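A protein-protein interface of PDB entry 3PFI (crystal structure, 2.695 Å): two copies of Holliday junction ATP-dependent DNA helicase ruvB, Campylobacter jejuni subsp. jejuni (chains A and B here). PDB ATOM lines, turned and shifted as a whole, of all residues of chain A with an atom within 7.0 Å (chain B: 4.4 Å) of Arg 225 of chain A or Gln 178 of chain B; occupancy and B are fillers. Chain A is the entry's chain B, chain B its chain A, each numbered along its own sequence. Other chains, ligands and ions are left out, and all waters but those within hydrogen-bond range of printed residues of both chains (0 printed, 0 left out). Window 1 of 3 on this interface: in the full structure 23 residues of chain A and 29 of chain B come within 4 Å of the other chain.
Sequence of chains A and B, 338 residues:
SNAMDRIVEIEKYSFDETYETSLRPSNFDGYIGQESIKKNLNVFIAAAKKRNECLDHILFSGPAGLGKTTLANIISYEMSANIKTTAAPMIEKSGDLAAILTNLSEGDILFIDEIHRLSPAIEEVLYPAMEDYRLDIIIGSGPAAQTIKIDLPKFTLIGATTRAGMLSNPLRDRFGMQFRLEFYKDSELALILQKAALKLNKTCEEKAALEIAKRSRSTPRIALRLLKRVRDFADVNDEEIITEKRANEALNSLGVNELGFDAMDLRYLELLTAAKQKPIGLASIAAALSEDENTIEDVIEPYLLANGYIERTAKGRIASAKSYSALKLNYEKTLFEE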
ATOM      1  N   LEU A 193     -22.421  10.549 -14.473  1.00  0.00           N
ATOM      2  CA  LEU A 193     -22.109  11.564 -13.470  1.00  0.00           C
ATOM      3  C   LEU A 193     -23.250  11.694 -12.457  1.00  0.00           C
ATOM      4  O   LEU A 193     -23.028  11.654 -11.248  1.00  0.00           O
ATOM      5  CB  LEU A 193     -21.830  12.916 -14.134  1.00  0.00           C
ATOM      6  CG  LEU A 193     -20.535  12.983 -14.948  1.00  0.00           C
ATOM      7  CD1 LEU A 193     -20.350  14.363 -15.585  1.00  0.00           C
ATOM      8  CD2 LEU A 193     -19.327  12.627 -14.073  1.00  0.00           C
ATOM      9  N   ILE A 212     -19.775  19.236 -17.335  1.00  0.00           N
ATOM     10  CA  ILE A 212     -18.649  18.440 -16.856  1.00  0.00           C
ATOM     11  C   ILE A 212     -18.287  17.419 -17.916  1.00  0.00           C
ATOM     12  O   ILE A 212     -17.114  17.216 -18.227  1.00  0.00           O
ATOM     13  CB  ILE A 212     -18.985  17.675 -15.564  1.00  0.00           C
ATOM     14  CG1 ILE A 212     -19.237  18.637 -14.401  1.00  0.00           C
ATOM     15  CG2 ILE A 212     -17.850  16.717 -15.186  1.00  0.00           C
ATOM     16  CD1 ILE A 212     -19.671  17.927 -13.112  1.00  0.00           C
ATOM     17  N   THR A 219     -14.261  10.929 -21.168  1.00  0.00           N
ATOM     18  CA  THR A 219     -13.656   9.839 -20.406  1.00  0.00           C
ATOM     19  C   THR A 219     -14.149   9.700 -18.948  1.00  0.00           C
ATOM     20  O   THR A 219     -13.844  10.527 -18.083  1.00  0.00           O
ATOM     21  CB  THR A 219     -12.137   9.999 -20.397  1.00  0.00           C
ATOM     22  OG1 THR A 219     -11.667  10.092 -21.750  1.00  0.00           O
ATOM     23  CG2 THR A 219     -11.476   8.812 -19.676  1.00  0.00           C
ATOM     24  N   PRO A 220     -14.897   8.628 -18.669  1.00  0.00           N
ATOM     25  CA  PRO A 220     -15.424   8.357 -17.337  1.00  0.00           C
ATOM     26  C   PRO A 220     -14.515   8.728 -16.167  1.00  0.00           C
ATOM     27  O   PRO A 220     -14.964   9.404 -15.237  1.00  0.00           O
ATOM     28  CB  PRO A 220     -15.647   6.846 -17.367  1.00  0.00           C
ATOM     29  CG  PRO A 220     -16.063   6.580 -18.765  1.00  0.00           C
ATOM     30  CD  PRO A 220     -15.344   7.613 -19.636  1.00  0.00           C
ATOM     31  N   ARG A 221     -13.255   8.306 -16.198  1.00  0.00           N
ATOM     32  CA  ARG A 221     -12.364   8.596 -15.075  1.00  0.00           C
ATOM     33  C   ARG A 221     -12.194  10.087 -14.863  1.00  0.00           C
ATOM     34  O   ARG A 221     -12.295  10.582 -13.746  1.00  0.00           O
ATOM     35  CB  ARG A 221     -11.007   7.930 -15.260  1.00  0.00           C
ATOM     36  CG  ARG A 221     -10.060   8.143 -14.083  1.00  0.00           C
ATOM     37  CD  ARG A 221      -8.871   7.231 -14.222  1.00  0.00           C
ATOM     38  NE  ARG A 221      -9.253   5.841 -13.987  1.00  0.00           N
ATOM     39  CZ  ARG A 221      -8.580   4.782 -14.426  1.00  0.00           C
ATOM     40  NH1 ARG A 221      -7.500   4.932 -15.183  1.00  0.00           N
ATOM     41  NH2 ARG A 221      -9.016   3.564 -14.139  1.00  0.00           N
ATOM     42  N   ILE A 222     -11.935  10.809 -15.939  1.00  0.00           N
ATOM     43  CA  ILE A 222     -11.784  12.244 -15.840  1.00  0.00           C
ATOM     44  C   ILE A 222     -13.098  12.865 -15.353  1.00  0.00           C
ATOM     45  O   ILE A 222     -13.118  13.652 -14.407  1.00  0.00           O
ATOM     46  CB  ILE A 222     -11.355  12.836 -17.179  1.00  0.00           C
ATOM     47  CG1 ILE A 222      -9.982  12.273 -17.566  1.00  0.00           C
ATOM     48  CG2 ILE A 222     -11.308  14.349 -17.097  1.00  0.00           C
ATOM     49  CD1 ILE A 222      -9.380  12.892 -18.819  1.00  0.00           C
ATOM     50  N   ALA A 223     -14.199  12.474 -15.985  1.00  0.00           N
ATOM     51  CA  ALA A 223     -15.507  12.990 -15.622  1.00  0.00           C
ATOM     52  C   ALA A 223     -15.728  12.863 -14.134  1.00  0.00           C
ATOM     53  O   ALA A 223     -16.022  13.852 -13.464  1.00  0.00           O
ATOM     54  CB  ALA A 223     -16.596  12.252 -16.381  1.00  0.00           C
ATOM     55  N   LEU A 224     -15.581  11.636 -13.629  1.00  0.00           N
ATOM     56  CA  LEU A 224     -15.773  11.333 -12.202  1.00  0.00           C
ATOM     57  C   LEU A 224     -14.895  12.212 -11.323  1.00  0.00           C
ATOM     58  O   LEU A 224     -15.367  12.789 -10.351  1.00  0.00           O
ATOM     59  CB  LEU A 224     -15.488   9.858 -11.943  1.00  0.00           C
ATOM     60  CG  LEU A 224     -16.573   8.861 -12.380  1.00  0.00           C
ATOM     61  CD1 LEU A 224     -17.296   9.298 -13.631  1.00  0.00           C
ATOM     62  CD2 LEU A 224     -15.974   7.471 -12.558  1.00  0.00           C
ATOM     63  N   ARG A 225     -13.619  12.303 -11.680  1.00  0.00           N
ATOM     64  CA  ARG A 225     -12.648  13.141 -10.973  1.00  0.00           C
ATOM     65  C   ARG A 225     -13.114  14.598 -10.919  1.00  0.00           C
ATOM     66  O   ARG A 225     -13.069  15.225  -9.863  1.00  0.00           O
ATOM     67  CB  ARG A 225     -11.274  13.008 -11.649  1.00  0.00           C
ATOM     68  CG  ARG A 225     -10.339  14.212 -11.542  1.00  0.00           C
ATOM     69  CD  ARG A 225      -9.171  14.025 -12.526  1.00  0.00           C
ATOM     70  NE  ARG A 225      -8.529  15.233 -13.072  1.00  0.00           N
ATOM     71  CZ  ARG A 225      -8.630  16.484 -12.618  1.00  0.00           C
ATOM     72  NH1 ARG A 225      -7.985  17.449 -13.256  1.00  0.00           N
ATOM     73  NH2 ARG A 225      -9.329  16.797 -11.534  1.00  0.00           N
ATOM     74  N   LEU A 226     -13.560  15.140 -12.047  1.00  0.00           N
ATOM     75  CA  LEU A 226     -14.031  16.523 -12.069  1.00  0.00           C
ATOM     76  C   LEU A 226     -15.290  16.682 -11.213  1.00  0.00           C
ATOM     77  O   LEU A 226     -15.501  17.722 -10.595  1.00  0.00           O
ATOM     78  CB  LEU A 226     -14.286  16.992 -13.508  1.00  0.00           C
ATOM     79  CG  LEU A 226     -13.020  17.114 -14.365  1.00  0.00           C
ATOM     80  CD1 LEU A 226     -13.342  17.328 -15.830  1.00  0.00           C
ATOM     81  CD2 LEU A 226     -12.124  18.233 -13.842  1.00  0.00           C
ATOM     82  N   LEU A 227     -16.121  15.644 -11.175  1.00  0.00           N
ATOM     83  CA  LEU A 227     -17.342  15.683 -10.383  1.00  0.00           C
ATOM     84  C   LEU A 227     -17.019  15.919  -8.920  1.00  0.00           C
ATOM     85  O   LEU A 227     -17.689  16.692  -8.245  1.00  0.00           O
ATOM     86  CB  LEU A 227     -18.116  14.370 -10.519  1.00  0.00           C
ATOM     87  CG  LEU A 227     -19.414  14.264  -9.709  1.00  0.00           C
ATOM     88  CD1 LEU A 227     -20.396  15.364 -10.113  1.00  0.00           C
ATOM     89  CD2 LEU A 227     -20.041  12.883  -9.882  1.00  0.00           C
ATOM     90  N   LYS A 228     -15.995  15.242  -8.423  1.00  0.00           N
ATOM     91  CA  LYS A 228     -15.615  15.394  -7.031  1.00  0.00           C
ATOM     92  C   LYS A 228     -15.111  16.806  -6.731  1.00  0.00           C
ATOM     93  O   LYS A 228     -15.334  17.330  -5.639  1.00  0.00           O
ATOM     94  CB  LYS A 228     -14.604  14.317  -6.627  1.00  0.00           C
ATOM     95  CG  LYS A 228     -15.232  12.926  -6.583  1.00  0.00           C
ATOM     96  CD  LYS A 228     -14.281  11.848  -6.069  1.00  0.00           C
ATOM     97  CE  LYS A 228     -13.152  11.558  -7.054  1.00  0.00           C
ATOM     98  NZ  LYS A 228     -12.246  10.482  -6.550  1.00  0.00           N
ATOM     99  N   ARG A 229     -14.449  17.433  -7.695  1.00  0.00           N
ATOM    100  CA  ARG A 229     -13.974  18.791  -7.482  1.00  0.00           C
ATOM    101  C   ARG A 229     -15.167  19.746  -7.427  1.00  0.00           C
ATOM    102  O   ARG A 229     -15.168  20.704  -6.652  1.00  0.00           O
ATOM    103  CB  ARG A 229     -13.013  19.232  -8.575  1.00  0.00           C
ATOM    104  CG  ARG A 229     -11.733  18.423  -8.735  1.00  0.00           C
ATOM    105  CD  ARG A 229     -10.856  18.328  -7.492  1.00  0.00           C
ATOM    106  NE  ARG A 229     -11.059  17.089  -6.736  1.00  0.00           N
ATOM    107  CZ  ARG A 229     -11.680  16.981  -5.569  1.00  0.00           C
ATOM    108  NH1 ARG A 229     -12.168  18.047  -4.956  1.00  0.00           N
ATOM    109  NH2 ARG A 229     -11.789  15.792  -4.997  1.00  0.00           N
ATOM    110  N   VAL A 230     -16.174  19.490  -8.257  1.00  0.00           N
ATOM    111  CA  VAL A 230     -17.380  20.309  -8.254  1.00  0.00           C
ATOM    112  C   VAL A 230     -18.172  20.050  -6.966  1.00  0.00           C
ATOM    113  O   VAL A 230     -18.791  20.969  -6.417  1.00  0.00           O
ATOM    114  CB  VAL A 230     -18.266  20.042  -9.480  1.00  0.00           C
ATOM    115  CG1 VAL A 230     -19.537  20.875  -9.403  1.00  0.00           C
ATOM    116  CG2 VAL A 230     -17.502  20.355 -10.756  1.00  0.00           C
ATOM    117  N   LEU A 254     -10.402  25.851 -11.798  1.00  0.00           N
ATOM    118  CA  LEU A 254      -9.359  24.835 -11.963  1.00  0.00           C
ATOM    119  C   LEU A 254      -8.606  25.005 -13.276  1.00  0.00           C
ATOM    120  O   LEU A 254      -7.547  24.410 -13.470  1.00  0.00           O
ATOM    121  CB  LEU A 254      -9.955  23.427 -11.910  1.00  0.00           C
ATOM    122  CG  LEU A 254     -10.355  22.920 -10.531  1.00  0.00           C
ATOM    123  CD1 LEU A 254     -11.155  21.632 -10.640  1.00  0.00           C
ATOM    124  CD2 LEU A 254      -9.106  22.725  -9.695  1.00  0.00           C
ATOM    125  N   VAL A 256      -9.742  24.081 -16.296  1.00  0.00           N
ATOM    126  CA  VAL A 256      -9.993  22.983 -17.222  1.00  0.00           C
ATOM    127  C   VAL A 256     -10.488  23.564 -18.546  1.00  0.00           C
ATOM    128  O   VAL A 256     -11.369  24.420 -18.565  1.00  0.00           O
ATOM    129  CB  VAL A 256     -11.059  22.005 -16.695  1.00  0.00           C
ATOM    130  CG1 VAL A 256     -11.261  20.876 -17.692  1.00  0.00           C
ATOM    131  CG2 VAL A 256     -10.670  21.444 -15.336  1.00  0.00           C
ATOM    132  N   LEU B  59      -1.571  16.343  -7.203  1.00  0.00           N
ATOM    133  CA  LEU B  59      -0.438  16.292  -8.106  1.00  0.00           C
ATOM    134  C   LEU B  59       0.036  17.700  -8.384  1.00  0.00           C
ATOM    135  O   LEU B  59      -0.754  18.552  -8.792  1.00  0.00           O
ATOM    136  CB  LEU B  59      -0.817  15.653  -9.438  1.00  0.00           C
ATOM    137  CG  LEU B  59       0.326  15.641 -10.459  1.00  0.00           C
ATOM    138  CD1 LEU B  59       1.413  14.677 -10.008  1.00  0.00           C
ATOM    139  CD2 LEU B  59      -0.161  15.274 -11.853  1.00  0.00           C
ATOM    140  N   ARG B 172      -1.739  10.219 -13.868  1.00  0.00           N
ATOM    141  CA  ARG B 172      -2.231  11.566 -13.559  1.00  0.00           C
ATOM    142  C   ARG B 172      -3.753  11.591 -13.381  1.00  0.00           C
ATOM    143  O   ARG B 172      -4.275  12.288 -12.500  1.00  0.00           O
ATOM    144  CB  ARG B 172      -1.794  12.612 -14.596  1.00  0.00           C
ATOM    145  CG  ARG B 172      -2.411  12.473 -15.971  1.00  0.00           C
ATOM    146  CD  ARG B 172      -2.137  13.711 -16.815  1.00  0.00           C
ATOM    147  NE  ARG B 172      -0.708  13.998 -16.938  1.00  0.00           N
ATOM    148  CZ  ARG B 172      -0.202  15.017 -17.630  1.00  0.00           C
ATOM    149  NH1 ARG B 172      -1.000  15.857 -18.280  1.00  0.00           N
ATOM    150  NH2 ARG B 172       1.112  15.196 -17.681  1.00  0.00           N
ATOM    151  N   ASP B 173      -4.460  10.814 -14.198  1.00  0.00           N
ATOM    152  CA  ASP B 173      -5.918  10.767 -14.120  1.00  0.00           C
ATOM    153  C   ASP B 173      -6.437  10.176 -12.804  1.00  0.00           C
ATOM    154  O   ASP B 173      -7.643  10.189 -12.558  1.00  0.00           O
ATOM    155  CB  ASP B 173      -6.498  10.018 -15.319  1.00  0.00           C
ATOM    156  CG  ASP B 173      -6.222  10.727 -16.633  1.00  0.00           C
ATOM    157  OD1 ASP B 173      -5.674  11.849 -16.596  1.00  0.00           O
ATOM    158  OD2 ASP B 173      -6.552  10.166 -17.698  1.00  0.00           O
ATOM    159  N   PHE B 175      -5.184  11.298  -9.854  1.00  0.00           N
ATOM    160  CA  PHE B 175      -5.028  12.361  -8.872  1.00  0.00           C
ATOM    161  C   PHE B 175      -6.274  13.215  -8.978  1.00  0.00           C
ATOM    162  O   PHE B 175      -6.551  13.782 -10.036  1.00  0.00           O
ATOM    163  CB  PHE B 175      -3.784  13.211  -9.139  1.00  0.00           C
ATOM    164  CG  PHE B 175      -2.497  12.521  -8.811  1.00  0.00           C
ATOM    165  CD1 PHE B 175      -1.969  12.593  -7.531  1.00  0.00           C
ATOM    166  CD2 PHE B 175      -1.811  11.813  -9.776  1.00  0.00           C
ATOM    167  CE1 PHE B 175      -0.783  11.959  -7.220  1.00  0.00           C
ATOM    168  CE2 PHE B 175      -0.621  11.177  -9.471  1.00  0.00           C
ATOM    169  CZ  PHE B 175      -0.109  11.249  -8.191  1.00  0.00           C
ATOM    170  N   GLY B 176      -7.040  13.288  -7.898  1.00  0.00           N
ATOM    171  CA  GLY B 176      -8.260  14.077  -7.896  1.00  0.00           C
ATOM    172  C   GLY B 176      -7.957  15.522  -8.219  1.00  0.00           C
ATOM    173  O   GLY B 176      -8.700  16.176  -8.943  1.00  0.00           O
ATOM    174  N   MET B 177      -6.842  16.002  -7.691  1.00  0.00           N
ATOM    175  CA  MET B 177      -6.406  17.375  -7.874  1.00  0.00           C
ATOM    176  C   MET B 177      -5.094  17.443  -8.646  1.00  0.00           C
ATOM    177  O   MET B 177      -4.140  16.722  -8.336  1.00  0.00           O
ATOM    178  CB  MET B 177      -6.250  18.039  -6.504  1.00  0.00           C
ATOM    179  CG  MET B 177      -7.575  18.430  -5.865  1.00  0.00           C
ATOM    180  SD  MET B 177      -7.482  18.612  -3.923  1.00  0.00           S
ATOM    181  CE  MET B 177      -7.440  16.707  -3.507  1.00  0.00           C
ATOM    182  N   GLN B 178      -5.069  18.315  -9.652  1.00  0.00           N
ATOM    183  CA  GLN B 178      -3.898  18.516 -10.492  1.00  0.00           C
ATOM    184  C   GLN B 178      -3.630  20.009 -10.581  1.00  0.00           C
ATOM    185  O   GLN B 178      -4.516  20.774 -10.950  1.00  0.00           O
ATOM    186  CB  GLN B 178      -4.152  17.948 -11.883  1.00  0.00           C
ATOM    187  CG  GLN B 178      -4.503  16.472 -11.869  1.00  0.00           C
ATOM    188  CD  GLN B 178      -4.894  15.928 -13.226  1.00  0.00           C
ATOM    189  OE1 GLN B 178      -5.309  14.776 -13.340  1.00  0.00           O
ATOM    190  NE2 GLN B 178      -4.776  16.752 -14.260  1.00  0.00           N
ATOM    191  N   PHE B 179      -2.416  20.420 -10.232  1.00  0.00           N
ATOM    192  CA  PHE B 179      -2.040  21.827 -10.270  1.00  0.00           C
ATOM    193  C   PHE B 179      -0.690  21.997 -10.931  1.00  0.00           C
ATOM    194  O   PHE B 179       0.249  21.257 -10.634  1.00  0.00           O
ATOM    195  CB  PHE B 179      -1.916  22.410  -8.863  1.00  0.00           C
ATOM    196  CG  PHE B 179      -3.164  22.317  -8.038  1.00  0.00           C
ATOM    197  CD1 PHE B 179      -4.277  23.071  -8.352  1.00  0.00           C
ATOM    198  CD2 PHE B 179      -3.195  21.530  -6.901  1.00  0.00           C
ATOM    199  CE1 PHE B 179      -5.415  23.003  -7.580  1.00  0.00           C
ATOM    200  CE2 PHE B 179      -4.325  21.465  -6.124  1.00  0.00           C
ATOM    201  CZ  PHE B 179      -5.436  22.201  -6.464  1.00  0.00           C
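No position is printed for both chains. Of the 6 pairs that touch across the chains among the printed residues, none has its exchanged pair printed and touching as well.
O of Gly 176 of chain B is in hydrogen-bond range of NH2 of Arg 225 of chain A. The backbone carbonyl oxygen (O) of Gly 176 of chain B is in hydrogen-bond range of the guanidinium group (NE) of Arg 229 of chain A (3.4 Å). The side-chain amide oxygen of Gln 178 of chain B lies within hydrogen-bond range of the guanidinium group of Arg 225 of chain A, at 3.3 Å.
Among the printed residues, pairs that only touch across the chains: Arg 221 of chain A with Asp 173 of chain B (3.5 Å), Arg 225 of chain A with Phe 175 of chain B (3.6 Å) and Arg 229 of chain A with Met 177 of chain B (3.7 Å).
Among the printed residues, 6 pairs touch across the chains.
The backbone NH (N) of Leu 59 of chain B lies within hydrogen-bond range of the backbone carbonyl oxygen (O) of Met 177 of chain B (2.8 Å). O of Arg 172 of chain B lies close to OE1 of Gln 178 of chain B (2.8 Å).
Of the printed residues of chain B, Arg 229 of chain A touches Gly 176 and Met 177. Of the printed residues of chain A, Asp 173 of chain B touches Arg 221 (3.5 Å). Of the printed residues of chain A, Met 177 of chain B touches Arg 229 (3.7 Å). Of the printed residues of chain A, Gly 176 of chain B touches Arg 225 and Arg 229. Printed residues of chain A within 4 Å of Phe 175 of chain B: Arg 225.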
